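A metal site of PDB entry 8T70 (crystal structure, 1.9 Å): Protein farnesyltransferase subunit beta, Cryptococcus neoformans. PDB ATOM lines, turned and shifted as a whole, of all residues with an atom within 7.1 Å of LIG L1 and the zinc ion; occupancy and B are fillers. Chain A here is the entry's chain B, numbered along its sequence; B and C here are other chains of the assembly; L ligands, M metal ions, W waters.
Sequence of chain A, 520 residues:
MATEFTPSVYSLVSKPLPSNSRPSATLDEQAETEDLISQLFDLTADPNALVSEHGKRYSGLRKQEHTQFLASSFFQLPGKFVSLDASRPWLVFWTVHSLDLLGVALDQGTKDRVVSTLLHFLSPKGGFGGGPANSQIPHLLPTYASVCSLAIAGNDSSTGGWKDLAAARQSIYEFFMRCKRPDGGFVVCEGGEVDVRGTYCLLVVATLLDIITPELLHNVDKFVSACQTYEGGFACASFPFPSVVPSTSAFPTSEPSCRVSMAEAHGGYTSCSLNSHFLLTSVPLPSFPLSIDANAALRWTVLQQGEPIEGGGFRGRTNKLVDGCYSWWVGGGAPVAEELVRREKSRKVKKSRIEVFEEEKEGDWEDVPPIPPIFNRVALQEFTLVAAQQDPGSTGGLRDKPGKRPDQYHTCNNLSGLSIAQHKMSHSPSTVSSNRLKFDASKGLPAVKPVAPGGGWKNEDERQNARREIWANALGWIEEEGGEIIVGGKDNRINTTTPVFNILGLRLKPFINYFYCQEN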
ATOM      1  N   HIS A 266      25.723  -8.772  25.149  1.00  0.00           N
ATOM      2  CA  HIS A 266      25.764  -9.077  23.722  1.00  0.00           C
ATOM      3  C   HIS A 266      25.219  -7.882  22.950  1.00  0.00           C
ATOM      4  O   HIS A 266      24.248  -7.243  23.373  1.00  0.00           O
ATOM      5  CB  HIS A 266      24.950 -10.331  23.400  1.00  0.00           C
ATOM      6  CG  HIS A 266      25.076 -10.773  21.976  1.00  0.00           C
ATOM      7  ND1 HIS A 266      25.953 -11.747  21.569  1.00  0.00           N
ATOM      8  CD2 HIS A 266      24.457 -10.334  20.850  1.00  0.00           C
ATOM      9  CE1 HIS A 266      25.856 -11.910  20.261  1.00  0.00           C
ATOM     10  NE2 HIS A 266      24.952 -11.057  19.796  1.00  0.00           N
ATOM     11  N   GLY A 268      23.452  -7.600  20.241  1.00  0.00           N
ATOM     12  CA  GLY A 268      22.034  -7.688  19.897  1.00  0.00           C
ATOM     13  C   GLY A 268      21.120  -7.356  21.062  1.00  0.00           C
ATOM     14  O   GLY A 268      20.189  -6.561  20.935  1.00  0.00           O
ATOM     15  N   TYR A 269      21.380  -7.966  22.223  1.00  0.00           N
ATOM     16  CA  TYR A 269      20.527  -7.691  23.374  1.00  0.00           C
ATOM     17  C   TYR A 269      20.848  -6.350  24.006  1.00  0.00           C
ATOM     18  O   TYR A 269      19.958  -5.754  24.635  1.00  0.00           O
ATOM     19  CB  TYR A 269      20.653  -8.835  24.384  1.00  0.00           C
ATOM     20  CG  TYR A 269      20.265 -10.170  23.790  1.00  0.00           C
ATOM     21  CD1 TYR A 269      18.974 -10.386  23.336  1.00  0.00           C
ATOM     22  CD2 TYR A 269      21.184 -11.204  23.674  1.00  0.00           C
ATOM     23  CE1 TYR A 269      18.610 -11.596  22.782  1.00  0.00           C
ATOM     24  CE2 TYR A 269      20.829 -12.409  23.123  1.00  0.00           C
ATOM     25  CZ  TYR A 269      19.543 -12.603  22.686  1.00  0.00           C
ATOM     26  OH  TYR A 269      19.187 -13.820  22.152  1.00  0.00           O
ATOM     27  N   GLY A 316      30.316  -8.466  18.747  1.00  0.00           N
ATOM     28  CA  GLY A 316      29.071  -8.517  19.491  1.00  0.00           C
ATOM     29  C   GLY A 316      29.260  -8.891  20.951  1.00  0.00           C
ATOM     30  O   GLY A 316      28.343  -8.700  21.758  1.00  0.00           O
ATOM     31  N   ASP A 323      31.920  -8.299  13.172  1.00  0.00           N
ATOM     32  CA  ASP A 323      30.851  -8.737  12.277  1.00  0.00           C
ATOM     33  C   ASP A 323      30.060  -7.504  11.865  1.00  0.00           C
ATOM     34  O   ASP A 323      29.617  -6.733  12.735  1.00  0.00           O
ATOM     35  CB  ASP A 323      29.967  -9.788  12.978  1.00  0.00           C
ATOM     36  CG  ASP A 323      28.737 -10.197  12.169  1.00  0.00           C
ATOM     37  OD1 ASP A 323      28.394  -9.543  11.147  1.00  0.00           O
ATOM     38  OD2 ASP A 323      28.095 -11.204  12.557  1.00  0.00           O
ATOM     39  N   GLY A 324      29.886  -7.320  10.554  1.00  0.00           N
ATOM     40  CA  GLY A 324      29.224  -6.133  10.041  1.00  0.00           C
ATOM     41  C   GLY A 324      27.837  -5.873  10.582  1.00  0.00           C
ATOM     42  O   GLY A 324      27.399  -4.724  10.617  1.00  0.00           O
ATOM     43  N   CYS A 325      27.099  -6.915  11.014  1.00  0.00           N
ATOM     44  CA  CYS A 325      25.747  -6.637  11.508  1.00  0.00           C
ATOM     45  C   CYS A 325      25.771  -5.870  12.825  1.00  0.00           C
ATOM     46  O   CYS A 325      24.797  -5.166  13.147  1.00  0.00           O
ATOM     47  CB  CYS A 325      24.901  -7.914  11.635  1.00  0.00           C
ATOM     48  SG  CYS A 325      25.427  -9.115  12.891  1.00  0.00           S
ATOM     49  N   TYR A 326      26.879  -5.937  13.585  1.00  0.00           N
ATOM     50  CA  TYR A 326      26.997  -5.163  14.813  1.00  0.00           C
ATOM     51  C   TYR A 326      27.292  -3.691  14.568  1.00  0.00           C
ATOM     52  O   TYR A 326      27.303  -2.911  15.525  1.00  0.00           O
ATOM     53  CB  TYR A 326      28.077  -5.753  15.729  1.00  0.00           C
ATOM     54  CG  TYR A 326      27.750  -7.160  16.141  1.00  0.00           C
ATOM     55  CD1 TYR A 326      26.558  -7.442  16.797  1.00  0.00           C
ATOM     56  CD2 TYR A 326      28.608  -8.212  15.849  1.00  0.00           C
ATOM     57  CE1 TYR A 326      26.239  -8.739  17.164  1.00  0.00           C
ATOM     58  CE2 TYR A 326      28.295  -9.516  16.212  1.00  0.00           C
ATOM     59  CZ  TYR A 326      27.109  -9.771  16.876  1.00  0.00           C
ATOM     60  OH  TYR A 326      26.800 -11.052  17.255  1.00  0.00           O
ATOM     61  N   TRP A 329      23.758  -3.073  15.577  1.00  0.00           N
ATOM     62  CA  TRP A 329      23.401  -3.446  16.952  1.00  0.00           C
ATOM     63  C   TRP A 329      24.242  -2.681  17.971  1.00  0.00           C
ATOM     64  O   TRP A 329      23.711  -2.187  18.973  1.00  0.00           O
ATOM     65  CB  TRP A 329      23.551  -4.954  17.166  1.00  0.00           C
ATOM     66  CG  TRP A 329      22.663  -5.746  16.261  1.00  0.00           C
ATOM     67  CD1 TRP A 329      23.037  -6.693  15.349  1.00  0.00           C
ATOM     68  CD2 TRP A 329      21.237  -5.615  16.145  1.00  0.00           C
ATOM     69  NE1 TRP A 329      21.928  -7.164  14.673  1.00  0.00           N
ATOM     70  CE2 TRP A 329      20.817  -6.530  15.148  1.00  0.00           C
ATOM     71  CE3 TRP A 329      20.279  -4.837  16.789  1.00  0.00           C
ATOM     72  CZ2 TRP A 329      19.482  -6.673  14.793  1.00  0.00           C
ATOM     73  CZ3 TRP A 329      18.944  -4.981  16.434  1.00  0.00           C
ATOM     74  CH2 TRP A 329      18.555  -5.883  15.435  1.00  0.00           C
ATOM     75  N   ARG A 399      27.790  -8.228   4.095  1.00  0.00           N
ATOM     76  CA  ARG A 399      28.072  -9.506   4.734  1.00  0.00           C
ATOM     77  C   ARG A 399      28.626  -9.288   6.127  1.00  0.00           C
ATOM     78  O   ARG A 399      28.974  -8.175   6.525  1.00  0.00           O
ATOM     79  CB  ARG A 399      29.066 -10.320   3.906  1.00  0.00           C
ATOM     80  CG  ARG A 399      30.399  -9.580   3.740  1.00  0.00           C
ATOM     81  CD  ARG A 399      31.304 -10.233   2.716  1.00  0.00           C
ATOM     82  NE  ARG A 399      32.545  -9.489   2.561  1.00  0.00           N
ATOM     83  CZ  ARG A 399      33.436  -9.717   1.604  1.00  0.00           C
ATOM     84  NH1 ARG A 399      33.267 -10.698   0.730  1.00  0.00           N
ATOM     85  NH2 ARG A 399      34.508  -8.943   1.524  1.00  0.00           N
ATOM     86  N   ASP A 400      28.687 -10.392   6.868  1.00  0.00           N
ATOM     87  CA  ASP A 400      29.298 -10.424   8.183  1.00  0.00           C
ATOM     88  C   ASP A 400      30.779 -10.032   8.108  1.00  0.00           C
ATOM     89  O   ASP A 400      31.222  -9.076   8.767  1.00  0.00           O
ATOM     90  CB  ASP A 400      29.076 -11.837   8.755  1.00  0.00           C
ATOM     91  CG  ASP A 400      30.067 -12.264   9.819  1.00  0.00           C
ATOM     92  OD1 ASP A 400      30.873 -11.477  10.350  1.00  0.00           O
ATOM     93  OD2 ASP A 400      30.013 -13.467  10.154  1.00  0.00           O
ATOM     94  N   LYS A 401      31.541 -10.741   7.295  1.00  0.00           N
ATOM     95  CA  LYS A 401      32.978 -10.488   7.156  1.00  0.00           C
ATOM     96  C   LYS A 401      33.429 -11.145   5.865  1.00  0.00           C
ATOM     97  O   LYS A 401      32.675 -11.929   5.264  1.00  0.00           O
ATOM     98  CB  LYS A 401      33.753 -11.029   8.388  1.00  0.00           C
ATOM     99  CG  LYS A 401      33.604 -12.515   8.593  1.00  0.00           C
ATOM    100  CD  LYS A 401      34.513 -13.062   9.715  1.00  0.00           C
ATOM    101  CE  LYS A 401      34.246 -12.408  11.062  1.00  0.00           C
ATOM    102  NZ  LYS A 401      32.942 -12.824  11.692  1.00  0.00           N
ATOM    103  N   ASP A 407      23.809 -11.553   2.807  1.00  0.00           N
ATOM    104  CA  ASP A 407      22.397 -11.904   2.927  1.00  0.00           C
ATOM    105  C   ASP A 407      21.622 -10.632   3.255  1.00  0.00           C
ATOM    106  O   ASP A 407      22.207  -9.567   3.470  1.00  0.00           O
ATOM    107  CB  ASP A 407      22.198 -13.027   3.962  1.00  0.00           C
ATOM    108  CG  ASP A 407      22.750 -12.686   5.344  1.00  0.00           C
ATOM    109  OD1 ASP A 407      22.575 -11.540   5.791  1.00  0.00           O
ATOM    110  OD2 ASP A 407      23.325 -13.575   6.002  1.00  0.00           O
ATOM    111  N   TYR A 409      19.810  -9.793   5.843  1.00  0.00           N
ATOM    112  CA  TYR A 409      20.008  -9.325   7.212  1.00  0.00           C
ATOM    113  C   TYR A 409      21.287  -8.492   7.342  1.00  0.00           C
ATOM    114  O   TYR A 409      21.266  -7.397   7.921  1.00  0.00           O
ATOM    115  CB  TYR A 409      20.051 -10.537   8.134  1.00  0.00           C
ATOM    116  CG  TYR A 409      20.639 -10.272   9.499  1.00  0.00           C
ATOM    117  CD1 TYR A 409      19.905  -9.602  10.469  1.00  0.00           C
ATOM    118  CD2 TYR A 409      21.919 -10.722   9.824  1.00  0.00           C
ATOM    119  CE1 TYR A 409      20.443  -9.376  11.744  1.00  0.00           C
ATOM    120  CE2 TYR A 409      22.457 -10.490  11.091  1.00  0.00           C
ATOM    121  CZ  TYR A 409      21.716  -9.813  12.041  1.00  0.00           C
ATOM    122  OH  TYR A 409      22.249  -9.562  13.296  1.00  0.00           O
ATOM    123  N   HIS A 410      22.405  -8.988   6.819  1.00  0.00           N
ATOM    124  CA  HIS A 410      23.649  -8.225   6.946  1.00  0.00           C
ATOM    125  C   HIS A 410      23.660  -7.034   6.012  1.00  0.00           C
ATOM    126  O   HIS A 410      24.318  -6.035   6.307  1.00  0.00           O
ATOM    127  CB  HIS A 410      24.864  -9.106   6.682  1.00  0.00           C
ATOM    128  CG  HIS A 410      25.117 -10.096   7.770  1.00  0.00           C
ATOM    129  ND1 HIS A 410      24.579 -11.362   7.757  1.00  0.00           N
ATOM    130  CD2 HIS A 410      25.805  -9.989   8.929  1.00  0.00           C
ATOM    131  CE1 HIS A 410      24.936 -12.007   8.849  1.00  0.00           C
ATOM    132  NE2 HIS A 410      25.691 -11.192   9.580  1.00  0.00           N
ATOM    133  N   ASN A 413      21.702  -4.454   8.135  1.00  0.00           N
ATOM    134  CA  ASN A 413      22.337  -3.981   9.356  1.00  0.00           C
ATOM    135  C   ASN A 413      23.678  -3.307   9.081  1.00  0.00           C
ATOM    136  O   ASN A 413      24.018  -2.327   9.753  1.00  0.00           O
ATOM    137  CB  ASN A 413      22.424  -5.136  10.356  1.00  0.00           C
ATOM    138  CG  ASN A 413      21.051  -5.411  10.973  1.00  0.00           C
ATOM    139  OD1 ASN A 413      20.520  -4.572  11.679  1.00  0.00           O
ATOM    140  ND2 ASN A 413      20.440  -6.530  10.632  1.00  0.00           N
ATOM    141  N   MET B   4      20.927 -15.767   9.238  1.00  0.00           N
ATOM    142  CA  MET B   4      20.063 -14.626   9.543  1.00  0.00           C
ATOM    143  C   MET B   4      19.133 -14.970  10.718  1.00  0.00           C
ATOM    144  O   MET B   4      17.980 -14.535  10.744  1.00  0.00           O
ATOM    145  CB  MET B   4      19.229 -14.220   8.311  1.00  0.00           C
ATOM    146  CG  MET B   4      19.995 -14.129   6.986  1.00  0.00           C
ATOM    147  SD  MET B   4      19.096 -13.167   5.715  1.00  0.00           S
ATOM    148  CE  MET B   4      18.968 -14.421   4.430  1.00  0.00           C
ATOM    149  N   ILE B   5      19.637 -15.740  11.678  1.00  0.00           N
ATOM    150  CA  ILE B   5      18.816 -16.286  12.764  1.00  0.00           C
ATOM    151  C   ILE B   5      18.805 -15.255  13.886  1.00  0.00           C
ATOM    152  O   ILE B   5      19.639 -15.263  14.787  1.00  0.00           O
ATOM    153  CB  ILE B   5      19.322 -17.650  13.242  1.00  0.00           C
ATOM    154  CG1 ILE B   5      19.379 -18.654  12.093  1.00  0.00           C
ATOM    155  CG2 ILE B   5      18.436 -18.178  14.375  1.00  0.00           C
ATOM    156  CD1 ILE B   5      19.991 -19.990  12.485  1.00  0.00           C
ATOM    157  N   ILE B   6      17.804 -14.372  13.843  1.00  0.00           N
ATOM    158  CA  ILE B   6      17.534 -13.454  14.947  1.00  0.00           C
ATOM    159  C   ILE B   6      16.206 -13.736  15.609  1.00  0.00           C
ATOM    160  O   ILE B   6      15.832 -13.012  16.547  1.00  0.00           O
ATOM    161  CB  ILE B   6      17.633 -11.978  14.500  1.00  0.00           C
ATOM    162  CG1 ILE B   6      16.917 -11.752  13.159  1.00  0.00           C
ATOM    163  CG2 ILE B   6      19.093 -11.565  14.390  1.00  0.00           C
ATOM    164  CD1 ILE B   6      15.413 -11.630  13.266  1.00  0.00           C
ATOM    165  N   TYR C 123      16.326 -20.840  18.358  1.00  0.00           N
ATOM    166  CA  TYR C 123      15.690 -20.298  19.573  1.00  0.00           C
ATOM    167  C   TYR C 123      14.561 -21.255  19.962  1.00  0.00           C
ATOM    168  O   TYR C 123      14.293 -21.398  21.149  1.00  0.00           O
ATOM    169  CB  TYR C 123      15.030 -18.953  19.283  1.00  0.00           C
ATOM    170  CG  TYR C 123      15.896 -17.727  19.428  1.00  0.00           C
ATOM    171  CD1 TYR C 123      16.085 -17.129  20.657  1.00  0.00           C
ATOM    172  CD2 TYR C 123      16.477 -17.145  18.320  1.00  0.00           C
ATOM    173  CE1 TYR C 123      16.870 -15.993  20.795  1.00  0.00           C
ATOM    174  CE2 TYR C 123      17.266 -16.017  18.430  1.00  0.00           C
ATOM    175  CZ  TYR C 123      17.460 -15.437  19.670  1.00  0.00           C
ATOM    176  OH  TYR C 123      18.234 -14.317  19.797  1.00  0.00           O
ATOM    177  N   HIS C 160      22.844 -19.353  23.309  1.00  0.00           N
ATOM    178  CA  HIS C 160      21.618 -19.970  23.812  1.00  0.00           C
ATOM    179  C   HIS C 160      21.927 -21.029  24.853  1.00  0.00           C
ATOM    180  O   HIS C 160      21.154 -21.231  25.793  1.00  0.00           O
ATOM    181  CB  HIS C 160      20.829 -20.621  22.667  1.00  0.00           C
ATOM    182  CG  HIS C 160      20.422 -19.686  21.583  1.00  0.00           C
ATOM    183  ND1 HIS C 160      19.865 -18.451  21.820  1.00  0.00           N
ATOM    184  CD2 HIS C 160      20.471 -19.816  20.230  1.00  0.00           C
ATOM    185  CE1 HIS C 160      19.595 -17.857  20.672  1.00  0.00           C
ATOM    186  NE2 HIS C 160      19.951 -18.666  19.685  1.00  0.00           N
HETATM  187  S1  LIG L   1      25.211 -12.906  12.343  1.00  0.00           S
HETATM  188  C1  LIG L   1      24.492 -13.004  13.996  1.00  0.00           C
HETATM  189  C2  LIG L   1      24.864 -12.111  14.988  1.00  0.00           C
HETATM  190  C3  LIG L   1      24.299 -12.214  16.251  1.00  0.00           C
HETATM  191  C4  LIG L   1      23.381 -13.213  16.485  1.00  0.00           C
HETATM  192  C5  LIG L   1      23.008 -14.113  15.501  1.00  0.00           C
HETATM  193  C6  LIG L   1      23.567 -14.003  14.242  1.00  0.00           C
HETATM  194  C1  LG2 L   2      15.321  -9.360  16.696  1.00  0.00           C
HETATM  195  C2  LG2 L   2      15.909  -8.048  17.221  1.00  0.00           C
HETATM  196  C3  LG2 L   2      15.072  -6.771  17.206  1.00  0.00           C
HETATM  197  C4  LG2 L   2      17.155  -8.018  17.701  1.00  0.00           C
HETATM  198  C5  LG2 L   2      18.019  -9.275  17.742  1.00  0.00           C
HETATM  199  C6  LG2 L   2      19.482  -8.810  17.645  1.00  0.00           C
HETATM  200  C7  LG2 L   2      20.512  -9.891  17.843  1.00  0.00           C
HETATM  201  C8  LG2 L   2      21.640 -10.014  16.824  1.00  0.00           C
HETATM  202  C9  LG2 L   2      20.475 -10.713  18.890  1.00  0.00           C
HETATM  203  C10 LG2 L   2      21.586 -11.774  19.070  1.00  0.00           C
HETATM  204  C11 LG2 L   2      21.032 -13.207  19.049  1.00  0.00           C
HETATM  205  C12 LG2 L   2      22.127 -14.223  19.468  1.00  0.00           C
HETATM  206  C13 LG2 L   2      22.957 -13.965  20.728  1.00  0.00           C
HETATM  207  C14 LG2 L   2      22.356 -15.308  18.759  1.00  0.00           C
HETATM  208  C15 LG2 L   2      23.450 -16.265  19.219  1.00  0.00           C
HETATM  209  O1  LG2 L   2      24.216 -16.735  18.122  1.00  0.00           O
HETATM  210  N1  LG2 L   2      24.947 -15.716  17.478  1.00  0.00           N
HETATM  211  C16 LG2 L   2      26.404 -15.624  17.581  1.00  0.00           C
HETATM  212  O2  LG2 L   2      27.022 -16.409  18.204  1.00  0.00           O
HETATM  213  C17 LG2 L   2      27.137 -14.505  16.836  1.00  0.00           C
HETATM  214  P1  LG2 L   2      28.572 -13.838  17.836  1.00  0.00           P
HETATM  215  O3  LG2 L   2      28.179 -13.478  19.250  1.00  0.00           O
HETATM  216  O4  LG2 L   2      29.749 -14.764  17.746  1.00  0.00           O
HETATM  217  O5  LG2 L   2      28.927 -12.548  17.134  1.00  0.00           O
HETATM  218 ZN    ZN M   1      26.231 -10.917  11.760  1.00  0.00          ZN
HETATM  219  O   HOH W   1      27.419 -14.691  10.365  1.00  0.00           O
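OH of Tyr 326 lies within hydrogen-bond range of NE2 of His 266 (3.1 Å).
N of Tyr 409 sits at hydrogen-bond distance from SD of Met 4 of chain B, 3.5 Å away.
N of Tyr 409 lies close to OD1 of Asp 407, at 3.3 Å.
OH of Tyr 409 sits at hydrogen-bond distance from NE1 of Trp 329, 2.8 Å away.
OH of Tyr 409 lies close to SG of Cys 325, 3.2 Å away.
N of His 410 sits at hydrogen-bond distance from OD1 of Asp 407, 2.8 Å away.
O of Tyr 409 is in hydrogen-bond range of ND2 of Asn 413 (3.0 Å).
The zinc ion is bound by the side-chain carboxylate of Asp 323 (2.0 Å), a ring nitrogen (NE2) of His 410 (2.3 Å), the side-chain sulfur of Cys 325 (2.3 Å) and a sulfur (S1) of LIG L1 (2.3 Å).
The zinc ion has four donor atoms within binding distance.
Slightly farther from the zinc ion lies OD1 of Asp 323 (2.6 Å).
Merely in contact with the zinc ion: Tyr 409 (3.9 Å).
Within 4 Å of the zinc ion: Asp 323, Cys 325, Tyr 409 and His 410.
Along chain A the residues within 4 Å of the zinc ion span positions 323 to 410.
An oxygen (O5) of LG2 L2 lies within hydrogen-bond range of the side-chain hydroxyl (OH) of Tyr 326, 2.6 Å away.
His 266 touches LIG L1 (NE2 to C3, 3.8 Å).
Tyr 326 touches LIG L1 (OH to C3, 2.9 Å).
Tyr 409 touches LIG L1.
Ile 5 of chain B touches LIG L1.
Hydrophobic or aromatic side chains that line LIG L1: Tyr 326, Tyr 409 and His 410.
Seven residues have an atom within 4 Å of LIG L1: His 266, Asp 323, Cys 325, Tyr 326, Tyr 409, His 410 and Ile 5 of chain B.
The nearest printed residue that does not touch LIG L1 is Ile 6 of chain B (4.8 Å).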
